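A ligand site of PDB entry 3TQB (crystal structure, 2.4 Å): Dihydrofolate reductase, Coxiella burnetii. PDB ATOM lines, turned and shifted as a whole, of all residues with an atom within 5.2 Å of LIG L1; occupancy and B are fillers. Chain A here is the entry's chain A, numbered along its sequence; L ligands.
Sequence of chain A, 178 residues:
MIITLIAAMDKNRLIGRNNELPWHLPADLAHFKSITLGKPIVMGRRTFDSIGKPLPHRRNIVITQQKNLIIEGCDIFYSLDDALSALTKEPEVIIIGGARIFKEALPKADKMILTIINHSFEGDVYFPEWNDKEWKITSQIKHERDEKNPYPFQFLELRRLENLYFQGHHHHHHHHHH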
ATOM      1  N   ILE A   6      25.051  25.344  15.719  1.00  0.00           N
ATOM      2  CA  ILE A   6      24.868  24.022  15.126  1.00  0.00           C
ATOM      3  C   ILE A   6      23.504  23.985  14.432  1.00  0.00           C
ATOM      4  O   ILE A   6      22.489  24.391  15.016  1.00  0.00           O
ATOM      5  CB  ILE A   6      24.973  22.909  16.193  1.00  0.00           C
ATOM      6  CG1 ILE A   6      24.869  21.525  15.544  1.00  0.00           C
ATOM      7  CG2 ILE A   6      23.914  23.077  17.284  1.00  0.00           C
ATOM      8  CD1 ILE A   6      25.107  20.376  16.504  1.00  0.00           C
ATOM      9  N   ALA A   7      23.485  23.526  13.188  1.00  0.00           N
ATOM     10  CA  ALA A   7      22.251  23.498  12.409  1.00  0.00           C
ATOM     11  C   ALA A   7      22.358  22.593  11.189  1.00  0.00           C
ATOM     12  O   ALA A   7      23.415  22.511  10.556  1.00  0.00           O
ATOM     13  CB  ALA A   7      21.877  24.904  11.965  1.00  0.00           C
ATOM     14  N   ALA A   8      21.264  21.904  10.882  1.00  0.00           N
ATOM     15  CA  ALA A   8      21.146  21.134   9.642  1.00  0.00           C
ATOM     16  C   ALA A   8      20.351  21.957   8.646  1.00  0.00           C
ATOM     17  O   ALA A   8      19.291  22.488   8.984  1.00  0.00           O
ATOM     18  CB  ALA A   8      20.457  19.808   9.907  1.00  0.00           C
ATOM     19  N   LEU A  21      10.960  19.969  11.309  1.00  0.00           N
ATOM     20  CA  LEU A  21      12.044  19.697  10.378  1.00  0.00           C
ATOM     21  C   LEU A  21      11.456  19.146   9.078  1.00  0.00           C
ATOM     22  O   LEU A  21      10.618  18.252   9.119  1.00  0.00           O
ATOM     23  CB  LEU A  21      13.027  18.674  10.962  1.00  0.00           C
ATOM     24  CG  LEU A  21      13.811  19.125  12.199  1.00  0.00           C
ATOM     25  CD1 LEU A  21      14.585  17.950  12.783  1.00  0.00           C
ATOM     26  CD2 LEU A  21      14.748  20.281  11.884  1.00  0.00           C
ATOM     27  N   TRP A  23      12.749  17.217   6.994  1.00  0.00           N
ATOM     28  CA  TRP A  23      13.356  15.921   6.677  1.00  0.00           C
ATOM     29  C   TRP A  23      13.520  15.084   7.949  1.00  0.00           C
ATOM     30  O   TRP A  23      13.142  15.502   9.038  1.00  0.00           O
ATOM     31  CB  TRP A  23      14.709  16.133   5.994  1.00  0.00           C
ATOM     32  CG  TRP A  23      15.679  16.927   6.831  1.00  0.00           C
ATOM     33  CD1 TRP A  23      16.445  16.471   7.863  1.00  0.00           C
ATOM     34  CD2 TRP A  23      15.957  18.327   6.708  1.00  0.00           C
ATOM     35  NE1 TRP A  23      17.190  17.492   8.391  1.00  0.00           N
ATOM     36  CE2 TRP A  23      16.916  18.643   7.699  1.00  0.00           C
ATOM     37  CE3 TRP A  23      15.515  19.339   5.854  1.00  0.00           C
ATOM     38  CZ2 TRP A  23      17.428  19.935   7.864  1.00  0.00           C
ATOM     39  CZ3 TRP A  23      16.020  20.620   6.007  1.00  0.00           C
ATOM     40  CH2 TRP A  23      16.971  20.909   7.012  1.00  0.00           C
ATOM     41  N   ASP A  28      22.353  12.529  11.069  1.00  0.00           N
ATOM     42  CA  ASP A  28      22.507  13.915  11.498  1.00  0.00           C
ATOM     43  C   ASP A  28      22.060  14.117  12.940  1.00  0.00           C
ATOM     44  O   ASP A  28      22.653  14.925  13.672  1.00  0.00           O
ATOM     45  CB  ASP A  28      21.709  14.839  10.567  1.00  0.00           C
ATOM     46  CG  ASP A  28      21.891  16.301  10.916  1.00  0.00           C
ATOM     47  OD1 ASP A  28      23.032  16.796  10.846  1.00  0.00           O
ATOM     48  OD2 ASP A  28      20.882  16.959  11.269  1.00  0.00           O
ATOM     49  N   LEU A  29      21.021  13.390  13.362  1.00  0.00           N
ATOM     50  CA  LEU A  29      20.515  13.479  14.730  1.00  0.00           C
ATOM     51  C   LEU A  29      21.473  12.848  15.746  1.00  0.00           C
ATOM     52  O   LEU A  29      21.568  13.310  16.876  1.00  0.00           O
ATOM     53  CB  LEU A  29      19.127  12.824  14.840  1.00  0.00           C
ATOM     54  CG  LEU A  29      18.027  13.472  14.007  1.00  0.00           C
ATOM     55  CD1 LEU A  29      16.749  12.639  14.062  1.00  0.00           C
ATOM     56  CD2 LEU A  29      17.749  14.891  14.481  1.00  0.00           C
ATOM     57  N   ALA A  30      22.174  11.790  15.330  1.00  0.00           N
ATOM     58  CA  ALA A  30      23.204  11.162  16.155  1.00  0.00           C
ATOM     59  C   ALA A  30      24.433  12.058  16.276  1.00  0.00           C
ATOM     60  O   ALA A  30      25.051  12.131  17.334  1.00  0.00           O
ATOM     61  CB  ALA A  30      23.591   9.803  15.579  1.00  0.00           C
ATOM     62  N   HIS A  31      24.767  12.719  15.174  1.00  0.00           N
ATOM     63  CA  HIS A  31      25.841  13.731  15.140  1.00  0.00           C
ATOM     64  C   HIS A  31      25.516  14.894  16.069  1.00  0.00           C
ATOM     65  O   HIS A  31      26.386  15.382  16.801  1.00  0.00           O
ATOM     66  CB  HIS A  31      26.047  14.221  13.702  1.00  0.00           C
ATOM     67  CG  HIS A  31      26.844  15.479  13.587  1.00  0.00           C
ATOM     68  ND1 HIS A  31      28.227  15.494  13.569  1.00  0.00           N
ATOM     69  CD2 HIS A  31      26.459  16.768  13.454  1.00  0.00           C
ATOM     70  CE1 HIS A  31      28.648  16.740  13.451  1.00  0.00           C
ATOM     71  NE2 HIS A  31      27.601  17.538  13.374  1.00  0.00           N
ATOM     72  N   PHE A  32      24.268  15.351  16.031  1.00  0.00           N
ATOM     73  CA  PHE A  32      23.792  16.418  16.903  1.00  0.00           C
ATOM     74  C   PHE A  32      23.888  16.032  18.396  1.00  0.00           C
ATOM     75  O   PHE A  32      24.210  16.876  19.229  1.00  0.00           O
ATOM     76  CB  PHE A  32      22.341  16.781  16.553  1.00  0.00           C
ATOM     77  CG  PHE A  32      21.727  17.805  17.470  1.00  0.00           C
ATOM     78  CD1 PHE A  32      21.875  19.158  17.224  1.00  0.00           C
ATOM     79  CD2 PHE A  32      20.998  17.392  18.577  1.00  0.00           C
ATOM     80  CE1 PHE A  32      21.308  20.103  18.077  1.00  0.00           C
ATOM     81  CE2 PHE A  32      20.421  18.329  19.429  1.00  0.00           C
ATOM     82  CZ  PHE A  32      20.581  19.678  19.176  1.00  0.00           C
ATOM     83  N   LYS A  33      23.607  14.771  18.707  1.00  0.00           N
ATOM     84  CA  LYS A  33      23.617  14.300  20.088  1.00  0.00           C
ATOM     85  C   LYS A  33      25.022  14.265  20.682  1.00  0.00           C
ATOM     86  O   LYS A  33      25.253  14.772  21.776  1.00  0.00           O
ATOM     87  CB  LYS A  33      22.971  12.915  20.196  1.00  0.00           C
ATOM     88  CG  LYS A  33      22.757  12.457  21.636  1.00  0.00           C
ATOM     89  CD  LYS A  33      21.836  11.244  21.720  1.00  0.00           C
ATOM     90  CE  LYS A  33      21.575  10.855  23.161  1.00  0.00           C
ATOM     91  NZ  LYS A  33      20.632   9.710  23.268  1.00  0.00           N
ATOM     92  N   THR A  36      26.413  17.867  21.178  1.00  0.00           N
ATOM     93  CA  THR A  36      25.754  18.669  22.210  1.00  0.00           C
ATOM     94  C   THR A  36      25.786  18.054  23.607  1.00  0.00           C
ATOM     95  O   THR A  36      25.469  18.732  24.580  1.00  0.00           O
ATOM     96  CB  THR A  36      24.275  18.932  21.848  1.00  0.00           C
ATOM     97  OG1 THR A  36      23.577  17.676  21.729  1.00  0.00           O
ATOM     98  CG2 THR A  36      24.181  19.693  20.541  1.00  0.00           C
ATOM     99  N   THR A  47      11.596  26.559  18.796  1.00  0.00           N
ATOM    100  CA  THR A  47      12.475  25.388  18.649  1.00  0.00           C
ATOM    101  C   THR A  47      12.228  24.379  19.765  1.00  0.00           C
ATOM    102  O   THR A  47      12.279  23.172  19.525  1.00  0.00           O
ATOM    103  CB  THR A  47      13.963  25.784  18.626  1.00  0.00           C
ATOM    104  OG1 THR A  47      14.220  26.626  17.493  1.00  0.00           O
ATOM    105  CG2 THR A  47      14.856  24.558  18.538  1.00  0.00           C
ATOM    106  N   SER A  50       9.210  22.620  18.854  1.00  0.00           N
ATOM    107  CA  SER A  50       9.575  21.687  17.797  1.00  0.00           C
ATOM    108  C   SER A  50      10.068  20.362  18.375  1.00  0.00           C
ATOM    109  O   SER A  50       9.705  19.296  17.873  1.00  0.00           O
ATOM    110  CB  SER A  50      10.649  22.298  16.882  1.00  0.00           C
ATOM    111  OG  SER A  50      11.258  21.318  16.050  1.00  0.00           O
ATOM    112  N   ILE A  51      10.884  20.432  19.418  1.00  0.00           N
ATOM    113  CA  ILE A  51      11.416  19.235  20.071  1.00  0.00           C
ATOM    114  C   ILE A  51      10.335  18.566  20.930  1.00  0.00           C
ATOM    115  O   ILE A  51      10.162  17.349  20.882  1.00  0.00           O
ATOM    116  CB  ILE A  51      12.664  19.546  20.918  1.00  0.00           C
ATOM    117  CG1 ILE A  51      13.787  20.081  20.024  1.00  0.00           C
ATOM    118  CG2 ILE A  51      13.138  18.308  21.655  1.00  0.00           C
ATOM    119  CD1 ILE A  51      15.042  20.490  20.768  1.00  0.00           C
ATOM    120  N   LEU A  55      15.917  18.112  25.966  1.00  0.00           N
ATOM    121  CA  LEU A  55      16.886  17.136  25.489  1.00  0.00           C
ATOM    122  C   LEU A  55      17.628  16.545  26.690  1.00  0.00           C
ATOM    123  O   LEU A  55      18.204  17.301  27.480  1.00  0.00           O
ATOM    124  CB  LEU A  55      17.885  17.783  24.528  1.00  0.00           C
ATOM    125  CG  LEU A  55      17.317  18.406  23.242  1.00  0.00           C
ATOM    126  CD1 LEU A  55      18.419  19.038  22.430  1.00  0.00           C
ATOM    127  CD2 LEU A  55      16.575  17.364  22.417  1.00  0.00           C
ATOM    128  N   PRO A  56      17.627  15.206  26.835  1.00  0.00           N
ATOM    129  CA  PRO A  56      18.205  14.632  28.050  1.00  0.00           C
ATOM    130  C   PRO A  56      19.721  14.796  28.148  1.00  0.00           C
ATOM    131  O   PRO A  56      20.392  14.933  27.118  1.00  0.00           O
ATOM    132  CB  PRO A  56      17.834  13.135  27.966  1.00  0.00           C
ATOM    133  CG  PRO A  56      17.042  12.961  26.714  1.00  0.00           C
ATOM    134  CD  PRO A  56      17.228  14.172  25.871  1.00  0.00           C
ATOM    135  N   ARG A  58      21.456  17.242  29.092  1.00  0.00           N
ATOM    136  CA  ARG A  58      21.896  18.559  28.632  1.00  0.00           C
ATOM    137  C   ARG A  58      21.123  19.670  29.336  1.00  0.00           C
ATOM    138  O   ARG A  58      19.918  19.538  29.592  1.00  0.00           O
ATOM    139  CB  ARG A  58      21.685  18.685  27.118  1.00  0.00           C
ATOM    140  CG  ARG A  58      22.840  18.152  26.296  1.00  0.00           C
ATOM    141  CD  ARG A  58      22.378  17.692  24.916  1.00  0.00           C
ATOM    142  NE  ARG A  58      21.567  16.482  24.995  1.00  0.00           N
ATOM    143  CZ  ARG A  58      21.128  15.800  23.948  1.00  0.00           C
ATOM    144  NH1 ARG A  58      21.411  16.193  22.708  1.00  0.00           N
ATOM    145  NH2 ARG A  58      20.398  14.704  24.131  1.00  0.00           N
ATOM    146  N   ILE A  96      21.451  26.516  18.988  1.00  0.00           N
ATOM    147  CA  ILE A  96      20.836  25.554  18.074  1.00  0.00           C
ATOM    148  C   ILE A  96      19.626  26.106  17.307  1.00  0.00           C
ATOM    149  O   ILE A  96      18.898  25.347  16.691  1.00  0.00           O
ATOM    150  CB  ILE A  96      20.429  24.252  18.823  1.00  0.00           C
ATOM    151  CG1 ILE A  96      19.217  24.480  19.739  1.00  0.00           C
ATOM    152  CG2 ILE A  96      21.590  23.725  19.643  1.00  0.00           C
ATOM    153  CD1 ILE A  96      18.746  23.233  20.444  1.00  0.00           C
ATOM    154  N   THR A 115      25.374  21.003   9.014  1.00  0.00           N
ATOM    155  CA  THR A 115      25.114  19.911   8.090  1.00  0.00           C
ATOM    156  C   THR A 115      24.403  20.462   6.853  1.00  0.00           C
ATOM    157  O   THR A 115      23.288  20.970   6.961  1.00  0.00           O
ATOM    158  CB  THR A 115      24.241  18.822   8.739  1.00  0.00           C
ATOM    159  OG1 THR A 115      24.811  18.440  10.000  1.00  0.00           O
ATOM    160  CG2 THR A 115      24.130  17.598   7.840  1.00  0.00           C
HETATM  161  N1  LIG L   1      21.217  20.548  14.253  1.00  0.00           N
HETATM  162  C1  LIG L   1      21.333  19.529  13.319  1.00  0.00           C
HETATM  163  N2  LIG L   1      22.516  19.246  12.781  1.00  0.00           N
HETATM  164  N3  LIG L   1      20.220  18.802  12.937  1.00  0.00           N
HETATM  165  C2  LIG L   1      18.982  19.074  13.478  1.00  0.00           C
HETATM  166  O1  LIG L   1      18.004  18.422  13.129  1.00  0.00           O
HETATM  167  C3  LIG L   1      18.854  20.105  14.417  1.00  0.00           C
HETATM  168  N4  LIG L   1      17.621  20.399  14.978  1.00  0.00           N
HETATM  169  C4  LIG L   1      17.506  21.407  15.904  1.00  0.00           C
HETATM  170  C5  LIG L   1      18.628  22.133  16.290  1.00  0.00           C
HETATM  171  N5  LIG L   1      19.859  21.851  15.737  1.00  0.00           N
HETATM  172  C6  LIG L   1      19.976  20.832  14.803  1.00  0.00           C
HETATM  173  C7  LIG L   1      16.178  21.746  16.531  1.00  0.00           C
HETATM  174  N6  LIG L   1      15.284  20.599  16.536  1.00  0.00           N
HETATM  175  C8  LIG L   1      16.172  16.860  18.044  1.00  0.00           C
HETATM  176  C9  LIG L   1      15.239  17.017  17.032  1.00  0.00           C
HETATM  177  C10 LIG L   1      14.946  18.291  16.536  1.00  0.00           C
HETATM  178  C11 LIG L   1      15.600  19.405  17.046  1.00  0.00           C
HETATM  179  C12 LIG L   1      16.553  19.246  18.065  1.00  0.00           C
HETATM  180  C13 LIG L   1      16.836  17.973  18.557  1.00  0.00           C
HETATM  181  C14 LIG L   1      16.457  15.477  18.559  1.00  0.00           C
HETATM  182  O2  LIG L   1      15.417  14.521  18.518  1.00  0.00           O
HETATM  183  N7  LIG L   1      17.669  15.189  19.025  1.00  0.00           N
HETATM  184  C15 LIG L   1      17.906  14.059  19.905  1.00  0.00           C
HETATM  185  C16 LIG L   1      18.238  12.817  19.081  1.00  0.00           C
HETATM  186  C17 LIG L   1      17.764  11.551  19.789  1.00  0.00           C
HETATM  187  C18 LIG L   1      18.214  10.312  19.049  1.00  0.00           C
HETATM  188  O3  LIG L   1      17.414   9.363  18.887  1.00  0.00           O
HETATM  189  O4  LIG L   1      19.372  10.209  18.596  1.00  0.00           O
HETATM  190  C19 LIG L   1      19.022  14.347  20.872  1.00  0.00           C
HETATM  191  O5  LIG L   1      19.720  15.376  20.756  1.00  0.00           O
HETATM  192  O6  LIG L   1      19.274  13.561  21.808  1.00  0.00           O
HETATM  193  P1  LG2 L   2      12.691  30.292  17.067  1.00  0.00           P
HETATM  194  O1  LG2 L   2      13.738  31.269  16.610  1.00  0.00           O
HETATM  195  O2  LG2 L   2      13.087  28.913  17.513  1.00  0.00           O
HETATM  196  O3  LG2 L   2      11.896  30.967  18.281  1.00  0.00           O
HETATM  197  C1  LG2 L   2      11.165  32.182  18.105  1.00  0.00           C
HETATM  198  C2  LG2 L   2      10.575  32.559  19.462  1.00  0.00           C
HETATM  199  O4  LG2 L   2      11.595  32.457  20.460  1.00  0.00           O
HETATM  200  C3  LG2 L   2      10.031  33.977  19.560  1.00  0.00           C
HETATM  201  O5  LG2 L   2       8.627  34.054  19.261  1.00  0.00           O
HETATM  202  C4  LG2 L   2      10.280  34.296  21.011  1.00  0.00           C
HETATM  203  O6  LG2 L   2       9.279  33.664  21.784  1.00  0.00           O
HETATM  204  C5  LG2 L   2      11.601  33.608  21.304  1.00  0.00           C
HETATM  205  N1  LG2 L   2      12.785  34.455  21.019  1.00  0.00           N
HETATM  206  C6  LG2 L   2      13.567  34.380  19.919  1.00  0.00           C
HETATM  207  N2  LG2 L   2      14.571  35.295  19.988  1.00  0.00           N
HETATM  208  C7  LG2 L   2      14.453  35.967  21.141  1.00  0.00           C
HETATM  209  C8  LG2 L   2      15.190  37.062  21.825  1.00  0.00           C
HETATM  210  N3  LG2 L   2      16.285  37.629  21.271  1.00  0.00           N
HETATM  211  N4  LG2 L   2      14.736  37.467  23.029  1.00  0.00           N
HETATM  212  C9  LG2 L   2      13.646  36.913  23.604  1.00  0.00           C
HETATM  213  N5  LG2 L   2      12.942  35.921  23.031  1.00  0.00           N
HETATM  214  C10 LG2 L   2      13.278  35.411  21.826  1.00  0.00           C
HETATM  215  O7  LG2 L   2      11.543  30.172  15.948  1.00  0.00           O
HETATM  216  P2  LG2 L   2      11.768  29.503  14.508  1.00  0.00           P
HETATM  217  O8  LG2 L   2      12.803  30.296  13.748  1.00  0.00           O
HETATM  218  O9  LG2 L   2      10.403  29.304  13.889  1.00  0.00           O
HETATM  219  O10 LG2 L   2      12.394  28.062  14.843  1.00  0.00           O
HETATM  220  C11 LG2 L   2      11.601  26.869  14.850  1.00  0.00           C
HETATM  221  C12 LG2 L   2      11.615  26.233  13.469  1.00  0.00           C
HETATM  222  O11 LG2 L   2      12.949  26.176  12.962  1.00  0.00           O
HETATM  223  C13 LG2 L   2      11.122  24.795  13.524  1.00  0.00           C
HETATM  224  O12 LG2 L   2      10.438  24.455  12.310  1.00  0.00           O
HETATM  225  C14 LG2 L   2      12.395  23.979  13.652  1.00  0.00           C
HETATM  226  O13 LG2 L   2      12.252  22.660  13.127  1.00  0.00           O
HETATM  227  C15 LG2 L   2      13.377  24.814  12.844  1.00  0.00           C
HETATM  228  N6  LG2 L   2      14.757  24.644  13.325  1.00  0.00           N
HETATM  229  C16 LG2 L   2      15.610  23.940  12.548  1.00  0.00           C
HETATM  230  C17 LG2 L   2      16.935  23.741  12.908  1.00  0.00           C
HETATM  231  C18 LG2 L   2      17.860  22.939  12.024  1.00  0.00           C
HETATM  232  O14 LG2 L   2      19.027  22.783  12.362  1.00  0.00           O
HETATM  233  N7  LG2 L   2      17.396  22.423  10.892  1.00  0.00           N
HETATM  234  C19 LG2 L   2      17.403  24.340  14.198  1.00  0.00           C
HETATM  235  C20 LG2 L   2      16.417  25.096  14.971  1.00  0.00           C
HETATM  236  C21 LG2 L   2      15.122  25.209  14.477  1.00  0.00           C
HETATM  237  P3  LG2 L   2       8.173  34.431  22.653  1.00  0.00           P
HETATM  238  O15 LG2 L   2       7.115  34.784  21.655  1.00  0.00           O
HETATM  239  O16 LG2 L   2       7.753  33.395  23.679  1.00  0.00           O
HETATM  240  O17 LG2 L   2       8.907  35.606  23.254  1.00  0.00           O
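The backbone NH of Ala 8 lies close to a nitrogen (N2) of LIG L1, at 3.5 Å. Ile 6 touches LIG L1. Ala 7 touches LIG L1. Leu 21 touches LIG L1. Leu 29 touches LIG L1 (CD2 to O1, 3.8 Å). Phe 32 touches LIG L1 (CD2 to O5, 3.2 Å). Lys 33 touches LIG L1. Thr 47 touches LIG L1 (CG2 to C7, 3.7 Å). Ile 51 touches LIG L1 (CD1 to C12, 3.3 Å). Leu 55 touches LIG L1. Ile 96 touches LIG L1 (O to C5, 3.3 Å). Thr 115 touches LIG L1 (OG1 to N2, 3.7 Å). Hydrophobic or aromatic side chains within 4 Å of LIG L1: Ile 6, Ala 8, Leu 21, Leu 29, Phe 32, Ile 51, Leu 55 and Ile 96. Within 4 Å of LIG L1: Ile 6, Ala 7, Ala 8, Leu 21, Asp 28, Leu 29, Phe 32, Lys 33, Thr 47, Ile 51, Leu 55, Arg 58, Ile 96 and Thr 115.
The side-chain hydroxyl (OG1) of Thr 47 is in hydrogen-bond range of an oxygen (O2) of LG2 L2 (2.6 Å). The backbone carbonyl oxygen (O) of Ala 8 sits at hydrogen-bond distance from a nitrogen (N7) of LG2 L2, at 2.7 Å. An oxygen (O14) of LG2 L2 is in hydrogen-bond range of the backbone NH of Ala 8 (2.8 Å). The backbone NH of Leu 21 lies within hydrogen-bond range of an oxygen (O13) of LG2 L2 (3.5 Å). The backbone NH (N) of Thr 47 lies within hydrogen-bond range of an oxygen (O2) of LG2 L2 (3.1 Å). The guanidinium group (NH1) of Arg 58 lies within salt-bridge range of an oxygen (O5) of LIG L1 (2.7 Å). An oxygen (O13) of LG2 L2 sits at hydrogen-bond distance from the side-chain hydroxyl of Ser 50, at 3.4 Å. N3 of LIG L1 lies within hydrogen-bond range of OD2 of Asp 28 (2.6 Å).
The backbone carbonyl oxygen (O) of Lys 33 lies within hydrogen-bond range of the side-chain hydroxyl (OG1) of Thr 36 (3.4 Å). The guanidinium group (NH1) of Arg 58 sits at hydrogen-bond distance from the side-chain hydroxyl (OG1) of Thr 36, at 2.8 Å. The side-chain carboxylate (OD1) of Asp 28 is in hydrogen-bond range of the side-chain hydroxyl (OG1) of Thr 115. The guanidinium group of Arg 58 sits at hydrogen-bond distance from the backbone carbonyl oxygen of Pro 56 (2.9 Å). The backbone carbonyl oxygen of Phe 32 sits at hydrogen-bond distance from the side-chain hydroxyl of Thr 36 (2.7 Å). N of Thr 115 is in hydrogen-bond range of O of Ala 7.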
